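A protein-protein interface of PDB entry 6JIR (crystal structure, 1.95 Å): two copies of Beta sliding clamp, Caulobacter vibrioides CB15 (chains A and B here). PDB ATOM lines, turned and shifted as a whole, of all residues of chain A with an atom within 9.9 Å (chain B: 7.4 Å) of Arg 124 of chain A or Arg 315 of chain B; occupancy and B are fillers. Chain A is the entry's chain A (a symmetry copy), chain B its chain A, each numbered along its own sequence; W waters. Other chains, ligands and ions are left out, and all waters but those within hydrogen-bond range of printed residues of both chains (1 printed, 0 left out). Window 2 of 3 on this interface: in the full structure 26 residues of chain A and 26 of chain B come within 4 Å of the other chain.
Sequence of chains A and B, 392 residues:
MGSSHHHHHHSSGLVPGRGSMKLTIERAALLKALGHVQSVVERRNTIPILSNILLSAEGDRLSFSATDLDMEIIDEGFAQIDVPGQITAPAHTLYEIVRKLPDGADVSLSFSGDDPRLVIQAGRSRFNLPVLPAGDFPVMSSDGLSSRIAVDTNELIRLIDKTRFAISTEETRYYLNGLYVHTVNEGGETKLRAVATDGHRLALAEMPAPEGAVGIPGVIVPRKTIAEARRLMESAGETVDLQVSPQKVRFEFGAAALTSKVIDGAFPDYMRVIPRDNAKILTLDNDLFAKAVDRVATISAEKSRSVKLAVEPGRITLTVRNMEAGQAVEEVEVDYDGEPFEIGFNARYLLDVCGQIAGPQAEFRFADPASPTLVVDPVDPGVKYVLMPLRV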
ATOM      1  N   LYS A 100      16.670   6.605 -12.173  1.00  0.00           N
ATOM      2  CA  LYS A 100      17.483   5.413 -12.412  1.00  0.00           C
ATOM      3  C   LYS A 100      18.840   5.681 -13.026  1.00  0.00           C
ATOM      4  O   LYS A 100      19.638   4.770 -13.127  1.00  0.00           O
ATOM      5  CB  LYS A 100      16.752   4.412 -13.298  1.00  0.00           C
ATOM      6  CG  LYS A 100      15.462   3.892 -12.748  1.00  0.00           C
ATOM      7  CD  LYS A 100      15.666   3.124 -11.468  1.00  0.00           C
ATOM      8  CE  LYS A 100      14.449   2.273 -11.129  1.00  0.00           C
ATOM      9  NZ  LYS A 100      14.781   1.443  -9.945  1.00  0.00           N
ATOM     10  N   LEU A 101      19.104   6.883 -13.509  1.00  0.00           N
ATOM     11  CA  LEU A 101      20.382   7.140 -14.173  1.00  0.00           C
ATOM     12  C   LEU A 101      21.496   7.113 -13.112  1.00  0.00           C
ATOM     13  O   LEU A 101      21.229   7.446 -11.958  1.00  0.00           O
ATOM     14  CB  LEU A 101      20.369   8.460 -14.930  1.00  0.00           C
ATOM     15  CG  LEU A 101      19.364   8.516 -16.081  1.00  0.00           C
ATOM     16  CD1 LEU A 101      19.328   9.918 -16.687  1.00  0.00           C
ATOM     17  CD2 LEU A 101      19.648   7.461 -17.160  1.00  0.00           C
ATOM     18  N   PRO A 102      22.728   6.707 -13.499  1.00  0.00           N
ATOM     19  CA  PRO A 102      23.781   6.607 -12.494  1.00  0.00           C
ATOM     20  C   PRO A 102      24.068   7.935 -11.797  1.00  0.00           C
ATOM     21  O   PRO A 102      24.068   8.995 -12.424  1.00  0.00           O
ATOM     22  CB  PRO A 102      25.007   6.142 -13.293  1.00  0.00           C
ATOM     23  CG  PRO A 102      24.471   5.531 -14.532  1.00  0.00           C
ATOM     24  CD  PRO A 102      23.219   6.325 -14.837  1.00  0.00           C
ATOM     25  N   ALA A 105      26.245  11.224 -13.257  1.00  0.00           N
ATOM     26  CA  ALA A 105      26.294  11.280 -14.720  1.00  0.00           C
ATOM     27  C   ALA A 105      25.669  12.567 -15.272  1.00  0.00           C
ATOM     28  O   ALA A 105      24.647  13.024 -14.790  1.00  0.00           O
ATOM     29  CB  ALA A 105      25.594  10.076 -15.305  1.00  0.00           C
ATOM     30  N   ASP A 106      26.322  13.181 -16.243  1.00  0.00           N
ATOM     31  CA  ASP A 106      25.753  14.321 -16.943  1.00  0.00           C
ATOM     32  C   ASP A 106      24.728  13.813 -17.961  1.00  0.00           C
ATOM     33  O   ASP A 106      24.965  12.822 -18.641  1.00  0.00           O
ATOM     34  CB  ASP A 106      26.839  15.168 -17.607  1.00  0.00           C
ATOM     35  CG  ASP A 106      27.331  16.299 -16.695  1.00  0.00           C
ATOM     36  OD1 ASP A 106      27.228  16.193 -15.444  1.00  0.00           O
ATOM     37  OD2 ASP A 106      27.815  17.301 -17.232  1.00  0.00           O
ATOM     38  N   ILE A 120      17.043  11.293 -24.230  1.00  0.00           N
ATOM     39  CA  ILE A 120      17.718  11.428 -22.946  1.00  0.00           C
ATOM     40  C   ILE A 120      18.864  10.417 -22.963  1.00  0.00           C
ATOM     41  O   ILE A 120      18.636   9.230 -23.161  1.00  0.00           O
ATOM     42  CB  ILE A 120      16.798  11.108 -21.757  1.00  0.00           C
ATOM     43  CG1 ILE A 120      15.548  11.985 -21.776  1.00  0.00           C
ATOM     44  CG2 ILE A 120      17.503  11.308 -20.421  1.00  0.00           C
ATOM     45  CD1 ILE A 120      14.340  11.269 -22.297  1.00  0.00           C
ATOM     46  N   GLN A 121      20.084  10.878 -22.762  1.00  0.00           N
ATOM     47  CA  GLN A 121      21.172   9.935 -22.544  1.00  0.00           C
ATOM     48  C   GLN A 121      22.194  10.349 -21.534  1.00  0.00           C
ATOM     49  O   GLN A 121      22.466  11.518 -21.335  1.00  0.00           O
ATOM     50  CB  GLN A 121      21.833   9.483 -23.827  1.00  0.00           C
ATOM     51  CG  GLN A 121      22.260  10.507 -24.811  1.00  0.00           C
ATOM     52  CD  GLN A 121      23.200   9.866 -25.838  1.00  0.00           C
ATOM     53  OE1 GLN A 121      22.812   9.544 -26.961  1.00  0.00           O
ATOM     54  NE2 GLN A 121      24.441   9.650 -25.429  1.00  0.00           N
ATOM     55  N   ALA A 122      22.690   9.317 -20.863  1.00  0.00           N
ATOM     56  CA  ALA A 122      23.659   9.413 -19.792  1.00  0.00           C
ATOM     57  C   ALA A 122      24.356   8.059 -19.770  1.00  0.00           C
ATOM     58  O   ALA A 122      23.706   7.028 -19.931  1.00  0.00           O
ATOM     59  CB  ALA A 122      22.975   9.673 -18.471  1.00  0.00           C
ATOM     60  N   GLY A 123      25.675   8.071 -19.613  1.00  0.00           N
ATOM     61  CA  GLY A 123      26.464   6.836 -19.637  1.00  0.00           C
ATOM     62  C   GLY A 123      26.246   6.073 -20.935  1.00  0.00           C
ATOM     63  O   GLY A 123      26.378   6.630 -22.006  1.00  0.00           O
ATOM     64  N   ARG A 124      25.826   4.818 -20.805  1.00  0.00           N
ATOM     65  CA  ARG A 124      25.563   3.921 -21.923  1.00  0.00           C
ATOM     66  C   ARG A 124      24.038   3.742 -22.223  1.00  0.00           C
ATOM     67  O   ARG A 124      23.688   2.862 -23.008  1.00  0.00           O
ATOM     68  CB  ARG A 124      26.174   2.546 -21.595  1.00  0.00           C
ATOM     69  CG  ARG A 124      27.621   2.583 -21.084  1.00  0.00           C
ATOM     70  CD  ARG A 124      28.556   3.149 -22.152  1.00  0.00           C
ATOM     71  NE  ARG A 124      28.470   2.322 -23.358  1.00  0.00           N
ATOM     72  CZ  ARG A 124      29.066   1.135 -23.524  1.00  0.00           C
ATOM     73  NH1 ARG A 124      29.840   0.610 -22.577  1.00  0.00           N
ATOM     74  NH2 ARG A 124      28.911   0.474 -24.666  1.00  0.00           N
ATOM     75  N   SER A 125      23.184   4.550 -21.578  1.00  0.00           N
ATOM     76  CA  SER A 125      21.718   4.523 -21.704  1.00  0.00           C
ATOM     77  C   SER A 125      21.239   5.555 -22.714  1.00  0.00           C
ATOM     78  O   SER A 125      21.749   6.662 -22.730  1.00  0.00           O
ATOM     79  CB  SER A 125      21.025   4.950 -20.396  1.00  0.00           C
ATOM     80  OG  SER A 125      21.371   4.180 -19.296  1.00  0.00           O
ATOM     81  N   ARG A 126      20.233   5.209 -23.506  1.00  0.00           N
ATOM     82  CA  ARG A 126      19.525   6.193 -24.324  1.00  0.00           C
ATOM     83  C   ARG A 126      18.023   5.933 -24.282  1.00  0.00           C
ATOM     84  O   ARG A 126      17.591   4.798 -24.498  1.00  0.00           O
ATOM     85  CB  ARG A 126      20.013   6.183 -25.774  1.00  0.00           C
ATOM     86  CG  ARG A 126      19.583   7.426 -26.543  1.00  0.00           C
ATOM     87  CD  ARG A 126      19.592   7.254 -28.044  1.00  0.00           C
ATOM     88  NE  ARG A 126      20.950   6.998 -28.496  1.00  0.00           N
ATOM     89  CZ  ARG A 126      21.375   5.920 -29.164  1.00  0.00           C
ATOM     90  NH1 ARG A 126      20.550   4.930 -29.536  1.00  0.00           N
ATOM     91  NH2 ARG A 126      22.665   5.847 -29.489  1.00  0.00           N
ATOM     92  N   PHE A 127      17.242   6.969 -23.963  1.00  0.00           N
ATOM     93  CA  PHE A 127      15.776   6.840 -23.928  1.00  0.00           C
ATOM     94  C   PHE A 127      15.232   7.828 -24.950  1.00  0.00           C
ATOM     95  O   PHE A 127      15.802   8.933 -25.085  1.00  0.00           O
ATOM     96  CB  PHE A 127      15.206   7.183 -22.543  1.00  0.00           C
ATOM     97  CG  PHE A 127      15.703   6.280 -21.427  1.00  0.00           C
ATOM     98  CD1 PHE A 127      16.987   6.438 -20.899  1.00  0.00           C
ATOM     99  CD2 PHE A 127      14.900   5.290 -20.918  1.00  0.00           C
ATOM    100  CE1 PHE A 127      17.436   5.613 -19.865  1.00  0.00           C
ATOM    101  CE2 PHE A 127      15.341   4.460 -19.894  1.00  0.00           C
ATOM    102  CZ  PHE A 127      16.614   4.620 -19.380  1.00  0.00           C
ATOM    103  N   LEU B 282      27.928 -17.172 -21.676  1.00  0.00           N
ATOM    104  CA  LEU B 282      28.090 -15.742 -21.586  1.00  0.00           C
ATOM    105  C   LEU B 282      28.300 -15.388 -20.114  1.00  0.00           C
ATOM    106  O   LEU B 282      27.481 -15.792 -19.272  1.00  0.00           O
ATOM    107  CB  LEU B 282      26.823 -15.030 -22.103  1.00  0.00           C
ATOM    108  CG  LEU B 282      26.885 -13.510 -22.217  1.00  0.00           C
ATOM    109  CD1 LEU B 282      26.073 -12.987 -23.423  1.00  0.00           C
ATOM    110  CD2 LEU B 282      26.439 -12.809 -20.920  1.00  0.00           C
ATOM    111  N   ARG B 295      17.105  -0.077 -15.339  1.00  0.00           N
ATOM    112  CA  ARG B 295      17.123   1.217 -15.954  1.00  0.00           C
ATOM    113  C   ARG B 295      16.279   1.201 -17.206  1.00  0.00           C
ATOM    114  O   ARG B 295      15.358   1.932 -17.323  1.00  0.00           O
ATOM    115  CB  ARG B 295      18.542   1.587 -16.313  1.00  0.00           C
ATOM    116  CG  ARG B 295      18.859   3.030 -16.422  1.00  0.00           C
ATOM    117  CD  ARG B 295      20.348   3.204 -16.611  1.00  0.00           C
ATOM    118  NE  ARG B 295      21.107   3.134 -15.370  1.00  0.00           N
ATOM    119  CZ  ARG B 295      22.127   2.332 -15.149  1.00  0.00           C
ATOM    120  NH1 ARG B 295      22.524   1.488 -16.043  1.00  0.00           N
ATOM    121  NH2 ARG B 295      22.746   2.381 -14.011  1.00  0.00           N
ATOM    122  N   VAL B 296      16.592   0.337 -18.147  1.00  0.00           N
ATOM    123  CA  VAL B 296      15.799   0.322 -19.393  1.00  0.00           C
ATOM    124  C   VAL B 296      14.342  -0.064 -19.188  1.00  0.00           C
ATOM    125  O   VAL B 296      13.479   0.418 -19.934  1.00  0.00           O
ATOM    126  CB  VAL B 296      16.402  -0.511 -20.560  1.00  0.00           C
ATOM    127  CG1 VAL B 296      17.691   0.134 -21.073  1.00  0.00           C
ATOM    128  CG2 VAL B 296      16.568  -1.998 -20.209  1.00  0.00           C
ATOM    129  N   LEU B 309      17.356  -8.909 -25.443  1.00  0.00           N
ATOM    130  CA  LEU B 309      18.825  -8.969 -25.332  1.00  0.00           C
ATOM    131  C   LEU B 309      19.331  -9.256 -26.736  1.00  0.00           C
ATOM    132  O   LEU B 309      19.063 -10.333 -27.255  1.00  0.00           O
ATOM    133  CB  LEU B 309      19.241 -10.120 -24.386  1.00  0.00           C
ATOM    134  CG  LEU B 309      19.160  -9.925 -22.865  1.00  0.00           C
ATOM    135  CD1 LEU B 309      17.756  -9.582 -22.399  1.00  0.00           C
ATOM    136  CD2 LEU B 309      19.668 -11.172 -22.129  1.00  0.00           C
ATOM    137  N   ALA B 310      20.062  -8.318 -27.335  1.00  0.00           N
ATOM    138  CA  ALA B 310      20.746  -8.560 -28.601  1.00  0.00           C
ATOM    139  C   ALA B 310      22.206  -8.867 -28.265  1.00  0.00           C
ATOM    140  O   ALA B 310      22.985  -7.983 -27.911  1.00  0.00           O
ATOM    141  CB  ALA B 310      20.632  -7.351 -29.539  1.00  0.00           C
ATOM    142  N   VAL B 311      22.560 -10.145 -28.388  1.00  0.00           N
ATOM    143  CA  VAL B 311      23.830 -10.650 -27.927  1.00  0.00           C
ATOM    144  C   VAL B 311      24.764 -10.734 -29.126  1.00  0.00           C
ATOM    145  O   VAL B 311      24.386 -11.268 -30.177  1.00  0.00           O
ATOM    146  CB  VAL B 311      23.673 -12.060 -27.321  1.00  0.00           C
ATOM    147  CG1 VAL B 311      24.990 -12.570 -26.765  1.00  0.00           C
ATOM    148  CG2 VAL B 311      22.593 -12.067 -26.244  1.00  0.00           C
ATOM    149  N   GLU B 312      25.976 -10.246 -28.944  1.00  0.00           N
ATOM    150  CA  GLU B 312      27.025 -10.398 -29.935  1.00  0.00           C
ATOM    151  C   GLU B 312      28.320 -10.612 -29.205  1.00  0.00           C
ATOM    152  O   GLU B 312      28.373 -10.376 -27.992  1.00  0.00           O
ATOM    153  CB  GLU B 312      27.115  -9.142 -30.822  1.00  0.00           C
ATOM    154  CG  GLU B 312      27.551  -7.885 -30.108  1.00  0.00           C
ATOM    155  CD  GLU B 312      27.462  -6.654 -30.997  1.00  0.00           C
ATOM    156  OE1 GLU B 312      26.496  -5.912 -30.875  1.00  0.00           O
ATOM    157  OE2 GLU B 312      28.360  -6.429 -31.812  1.00  0.00           O
ATOM    158  N   PRO B 313      29.395 -10.996 -29.930  1.00  0.00           N
ATOM    159  CA  PRO B 313      30.697 -11.068 -29.260  1.00  0.00           C
ATOM    160  C   PRO B 313      31.016  -9.803 -28.458  1.00  0.00           C
ATOM    161  O   PRO B 313      30.955  -8.687 -28.999  1.00  0.00           O
ATOM    162  CB  PRO B 313      31.696 -11.253 -30.420  1.00  0.00           C
ATOM    163  CG  PRO B 313      30.911 -11.927 -31.486  1.00  0.00           C
ATOM    164  CD  PRO B 313      29.450 -11.549 -31.298  1.00  0.00           C
ATOM    165  N   GLY B 314      31.300  -9.980 -27.160  1.00  0.00           N
ATOM    166  CA  GLY B 314      31.719  -8.885 -26.308  1.00  0.00           C
ATOM    167  C   GLY B 314      30.622  -7.937 -25.785  1.00  0.00           C
ATOM    168  O   GLY B 314      30.928  -7.022 -25.019  1.00  0.00           O
ATOM    169  N   ARG B 315      29.389  -8.122 -26.215  1.00  0.00           N
ATOM    170  CA  ARG B 315      28.336  -7.219 -25.818  1.00  0.00           C
ATOM    171  C   ARG B 315      26.902  -7.691 -25.872  1.00  0.00           C
ATOM    172  O   ARG B 315      26.539  -8.509 -26.638  1.00  0.00           O
ATOM    173  CB  ARG B 315      28.452  -5.971 -26.706  1.00  0.00           C
ATOM    174  CG  ARG B 315      27.348  -4.940 -26.600  1.00  0.00           C
ATOM    175  CD  ARG B 315      27.617  -3.726 -27.482  1.00  0.00           C
ATOM    176  NE  ARG B 315      28.843  -3.039 -27.126  1.00  0.00           N
ATOM    177  CZ  ARG B 315      29.464  -2.138 -27.881  1.00  0.00           C
ATOM    178  NH1 ARG B 315      28.983  -1.786 -29.053  1.00  0.00           N
ATOM    179  NH2 ARG B 315      30.572  -1.575 -27.451  1.00  0.00           N
ATOM    180  N   ILE B 316      26.090  -7.090 -25.032  1.00  0.00           N
ATOM    181  CA  ILE B 316      24.677  -7.296 -25.039  1.00  0.00           C
ATOM    182  C   ILE B 316      24.043  -5.929 -25.139  1.00  0.00           C
ATOM    183  O   ILE B 316      24.322  -5.097 -24.364  1.00  0.00           O
ATOM    184  CB  ILE B 316      24.110  -7.953 -23.759  1.00  0.00           C
ATOM    185  CG1 ILE B 316      24.523  -9.398 -23.640  1.00  0.00           C
ATOM    186  CG2 ILE B 316      22.588  -7.921 -23.730  1.00  0.00           C
ATOM    187  CD1 ILE B 316      24.014 -10.055 -22.405  1.00  0.00           C
ATOM    188  N   THR B 317      23.197  -5.734 -26.117  1.00  0.00           N
ATOM    189  CA  THR B 317      22.342  -4.534 -26.207  1.00  0.00           C
ATOM    190  C   THR B 317      20.944  -4.862 -25.698  1.00  0.00           C
ATOM    191  O   THR B 317      20.274  -5.745 -26.236  1.00  0.00           O
ATOM    192  CB  THR B 317      22.288  -3.987 -27.646  1.00  0.00           C
ATOM    193  OG1 THR B 317      23.629  -3.802 -28.081  1.00  0.00           O
ATOM    194  CG2 THR B 317      21.590  -2.639 -27.697  1.00  0.00           C
ATOM    195  N   LEU B 318      20.517  -4.117 -24.681  1.00  0.00           N
ATOM    196  CA  LEU B 318      19.217  -4.278 -24.045  1.00  0.00           C
ATOM    197  C   LEU B 318      18.240  -3.234 -24.584  1.00  0.00           C
ATOM    198  O   LEU B 318      18.569  -2.031 -24.599  1.00  0.00           O
ATOM    199  CB  LEU B 318      19.340  -4.036 -22.559  1.00  0.00           C
ATOM    200  CG  LEU B 318      20.238  -4.978 -21.777  1.00  0.00           C
ATOM    201  CD1 LEU B 318      20.604  -4.360 -20.435  1.00  0.00           C
ATOM    202  CD2 LEU B 318      19.506  -6.268 -21.622  1.00  0.00           C
ATOM    203  N   VAL B 329      17.356   1.928 -24.557  1.00  0.00           N
ATOM    204  CA  VAL B 329      18.428   1.076 -25.060  1.00  0.00           C
ATOM    205  C   VAL B 329      19.661   1.296 -24.207  1.00  0.00           C
ATOM    206  O   VAL B 329      19.990   2.426 -23.900  1.00  0.00           O
ATOM    207  CB  VAL B 329      18.791   1.380 -26.532  1.00  0.00           C
ATOM    208  CG1 VAL B 329      19.885   0.437 -27.038  1.00  0.00           C
ATOM    209  CG2 VAL B 329      17.563   1.262 -27.429  1.00  0.00           C
ATOM    210  N   GLU B 330      20.322   0.193 -23.824  1.00  0.00           N
ATOM    211  CA  GLU B 330      21.598   0.249 -23.145  1.00  0.00           C
ATOM    212  C   GLU B 330      22.528  -0.900 -23.572  1.00  0.00           C
ATOM    213  O   GLU B 330      22.104  -2.047 -23.713  1.00  0.00           O
ATOM    214  CB  GLU B 330      21.412   0.280 -21.623  1.00  0.00           C
ATOM    215  CG  GLU B 330      22.731   0.360 -20.818  1.00  0.00           C
ATOM    216  CD  GLU B 330      22.571   0.881 -19.399  1.00  0.00           C
ATOM    217  OE1 GLU B 330      21.435   1.180 -18.994  1.00  0.00           O
ATOM    218  OE2 GLU B 330      23.579   1.017 -18.668  1.00  0.00           O
ATOM    219  N   GLU B 331      23.800  -0.557 -23.761  1.00  0.00           N
ATOM    220  CA  GLU B 331      24.849  -1.520 -24.102  1.00  0.00           C
ATOM    221  C   GLU B 331      25.604  -1.912 -22.846  1.00  0.00           C
ATOM    222  O   GLU B 331      26.005  -1.046 -22.072  1.00  0.00           O
ATOM    223  CB  GLU B 331      25.832  -0.886 -25.091  1.00  0.00           C
ATOM    224  CG  GLU B 331      25.192  -0.655 -26.448  1.00  0.00           C
ATOM    225  CD  GLU B 331      26.118   0.020 -27.436  1.00  0.00           C
ATOM    226  OE1 GLU B 331      27.198   0.468 -27.053  1.00  0.00           O
ATOM    227  OE2 GLU B 331      25.749   0.091 -28.604  1.00  0.00           O
ATOM    228  N   VAL B 332      25.804  -3.213 -22.675  1.00  0.00           N
ATOM    229  CA  VAL B 332      26.570  -3.752 -21.561  1.00  0.00           C
ATOM    230  C   VAL B 332      27.670  -4.651 -22.158  1.00  0.00           C
ATOM    231  O   VAL B 332      27.363  -5.586 -22.893  1.00  0.00           O
ATOM    232  CB  VAL B 332      25.655  -4.540 -20.591  1.00  0.00           C
ATOM    233  CG1 VAL B 332      26.463  -5.204 -19.477  1.00  0.00           C
ATOM    234  CG2 VAL B 332      24.615  -3.607 -19.953  1.00  0.00           C
ATOM    235  N   GLU B 333      28.927  -4.343 -21.870  1.00  0.00           N
ATOM    236  CA  GLU B 333      30.033  -5.250 -22.258  1.00  0.00           C
ATOM    237  C   GLU B 333      29.983  -6.522 -21.409  1.00  0.00           C
ATOM    238  O   GLU B 333      29.678  -6.470 -20.217  1.00  0.00           O
ATOM    239  CB  GLU B 333      31.407  -4.581 -22.163  1.00  0.00           C
ATOM    240  CG  GLU B 333      31.822  -3.818 -23.427  1.00  0.00           C
ATOM    241  CD  GLU B 333      31.015  -2.548 -23.606  1.00  0.00           C
ATOM    242  OE1 GLU B 333      30.312  -2.389 -24.643  1.00  0.00           O
ATOM    243  OE2 GLU B 333      31.060  -1.716 -22.672  1.00  0.00           O
ATOM    244  N   VAL B 334      30.199  -7.655 -22.075  1.00  0.00           N
ATOM    245  CA  VAL B 334      30.143  -8.962 -21.486  1.00  0.00           C
ATOM    246  C   VAL B 334      31.280  -9.862 -22.080  1.00  0.00           C
ATOM    247  O   VAL B 334      31.919  -9.511 -23.075  1.00  0.00           O
ATOM    248  CB  VAL B 334      28.787  -9.637 -21.726  1.00  0.00           C
ATOM    249  CG1 VAL B 334      27.616  -8.798 -21.157  1.00  0.00           C
ATOM    250  CG2 VAL B 334      28.534  -9.938 -23.201  1.00  0.00           C
ATOM    251  N   ASP B 335      31.496 -11.005 -21.452  1.00  0.00           N
ATOM    252  CA  ASP B 335      32.415 -12.033 -21.976  1.00  0.00           C
ATOM    253  C   ASP B 335      31.628 -13.065 -22.789  1.00  0.00           C
ATOM    254  O   ASP B 335      30.893 -13.901 -22.257  1.00  0.00           O
ATOM    255  CB  ASP B 335      33.228 -12.681 -20.840  1.00  0.00           C
ATOM    256  CG  ASP B 335      34.227 -13.725 -21.360  1.00  0.00           C
ATOM    257  OD1 ASP B 335      34.839 -13.498 -22.411  1.00  0.00           O
ATOM    258  OD2 ASP B 335      34.415 -14.774 -20.714  1.00  0.00           O
ATOM    259  N   TYR B 336      31.723 -12.966 -24.115  1.00  0.00           N
ATOM    260  CA  TYR B 336      31.036 -13.913 -24.994  1.00  0.00           C
ATOM    261  C   TYR B 336      31.738 -13.877 -26.359  1.00  0.00           C
ATOM    262  O   TYR B 336      31.987 -12.820 -26.880  1.00  0.00           O
ATOM    263  CB  TYR B 336      29.546 -13.538 -25.141  1.00  0.00           C
ATOM    264  CG  TYR B 336      28.788 -14.388 -26.131  1.00  0.00           C
ATOM    265  CD1 TYR B 336      28.479 -15.699 -25.838  1.00  0.00           C
ATOM    266  CD2 TYR B 336      28.410 -13.897 -27.399  1.00  0.00           C
ATOM    267  CE1 TYR B 336      27.792 -16.492 -26.725  1.00  0.00           C
ATOM    268  CE2 TYR B 336      27.722 -14.703 -28.300  1.00  0.00           C
ATOM    269  CZ  TYR B 336      27.427 -15.995 -27.963  1.00  0.00           C
ATOM    270  OH  TYR B 336      26.724 -16.827 -28.801  1.00  0.00           O
ATOM    271  N   PHE B 341      22.757 -13.424 -31.613  1.00  0.00           N
ATOM    272  CA  PHE B 341      21.367 -13.820 -31.551  1.00  0.00           C
ATOM    273  C   PHE B 341      20.594 -12.804 -30.718  1.00  0.00           C
ATOM    274  O   PHE B 341      21.196 -12.010 -30.020  1.00  0.00           O
ATOM    275  CB  PHE B 341      21.201 -15.233 -30.981  1.00  0.00           C
ATOM    276  CG  PHE B 341      21.668 -15.394 -29.542  1.00  0.00           C
ATOM    277  CD1 PHE B 341      22.992 -15.651 -29.258  1.00  0.00           C
ATOM    278  CD2 PHE B 341      20.759 -15.330 -28.482  1.00  0.00           C
ATOM    279  CE1 PHE B 341      23.431 -15.832 -27.953  1.00  0.00           C
ATOM    280  CE2 PHE B 341      21.190 -15.493 -27.169  1.00  0.00           C
ATOM    281  CZ  PHE B 341      22.527 -15.744 -26.898  1.00  0.00           C
HETATM  282  O   HOH W   1      24.696   3.410 -18.116  1.00  0.00           O
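N of Leu 318 of chain B is in hydrogen-bond range of O of Glu 330 of chain B (2.8 Å). O of Ile 120 of chain A is in hydrogen-bond range of N of Phe 127 of chain A, at 2.8 Å. NH1 of Arg 315 of chain B is in salt-bridge range of OE1 of Glu 331 of chain B. NH1 of Arg 295 of chain B is in salt-bridge range of OE2 of Glu 330 of chain B (2.9 Å). OE1 of Glu 333 of chain B is in salt-bridge range of NH2 of Arg 315 of chain B (2.9 Å).
Among the printed residues, pairs that only touch across the chains: Pro 102 of chain A with Arg 295 of chain B, Arg 124 of chain A with Arg 315 of chain B, Arg 124 of chain A with Val 329 of chain B, Arg 124 of chain A with Glu 330 of chain B, Ser 125 of chain A with Arg 295 of chain B, Ser 125 of chain A with Val 329 of chain B and Phe 127 of chain A with Arg 295 of chain B.
Water W1 lies within hydrogen-bond range of OE2 of Glu 330 of chain B (2.7 Å) and N of Arg 124 of chain A (3.2 Å).
No position is printed for both chains.
Printed residues of chain A that touch a printed residue of chain B: Lys 100, Pro 102, Arg 124, Ser 125, Arg 126 and Phe 127. Hydrophobic or aromatic side chains of chain A that line the printed part of chain B: Pro 102 and Phe 127. Printed residues of chain B that touch a printed residue of chain A: Arg 295, Arg 315, Val 329, Glu 330, Glu 331 and Glu 333. Among the printed residues, 12 pairs touch across the chains. Among the printed residues, Asp or Glu carboxylates within 4 Å of a Lys or Arg side-chain nitrogen of the other chain: Arg 124 of chain A with Glu 331 of chain B (2.9 Å) and Arg 124 of chain A with Glu 333 of chain B (2.6 Å).
The backbone carbonyl oxygen (O) of Lys 100 of chain A lies within hydrogen-bond range of the guanidinium group (NE) of Arg 295 of chain B, at 3.1 Å. N of Arg 126 of chain A lies within hydrogen-bond range of O of Val 329 of chain B, at 2.8 Å. The side-chain carboxylate (OE2) of Glu 333 of chain B is in salt-bridge range of the guanidinium group (NH1) of Arg 124 of chain A (2.6 Å). OE1 of Glu 331 of chain B lies within salt-bridge range of NH2 of Arg 124 of chain A (2.9 Å). OE1 of Glu 330 of chain B lies within hydrogen-bond range of OG of Ser 125 of chain A (3.0 Å).
Of chain B, only Arg 315, Val 329, Glu 330, Glu 331 and Glu 333 come within 4 Å of Arg 124 of chain A. Of the printed residues of chain B, Phe 127 of chain A touches Arg 295 (3.6 Å). No residue of chain A comes within 4 Å of Val 311 of chain B. No residue of chain A comes within 4 Å of Glu 312 of chain B. No residue of chain A comes within 4 Å of Gly 314 of chain B. Arg 315 of chain B touches one residue of chain A. No residue of chain A comes within 4 Å of Ile 316 of chain B. Printed residues of chain A within 4 Å of Val 329 of chain B: Arg 124, Ser 125 and Arg 126. Glu 330 of chain B touches just these residues of chain A: Arg 124 (3.3 Å) and Ser 125 (3.0 Å). Glu 331 of chain B touches one residue of chain A. Glu 333 of chain B touches just one residue of chain A: Arg 124. The nearest printed residue of chain A that does not touch Arg 315 of chain B is Arg 126 of chain A (9.9 Å). The nearest printed residue of chain A that does not touch Val 329 of chain B is Phe 127 of chain A (5.1 Å).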
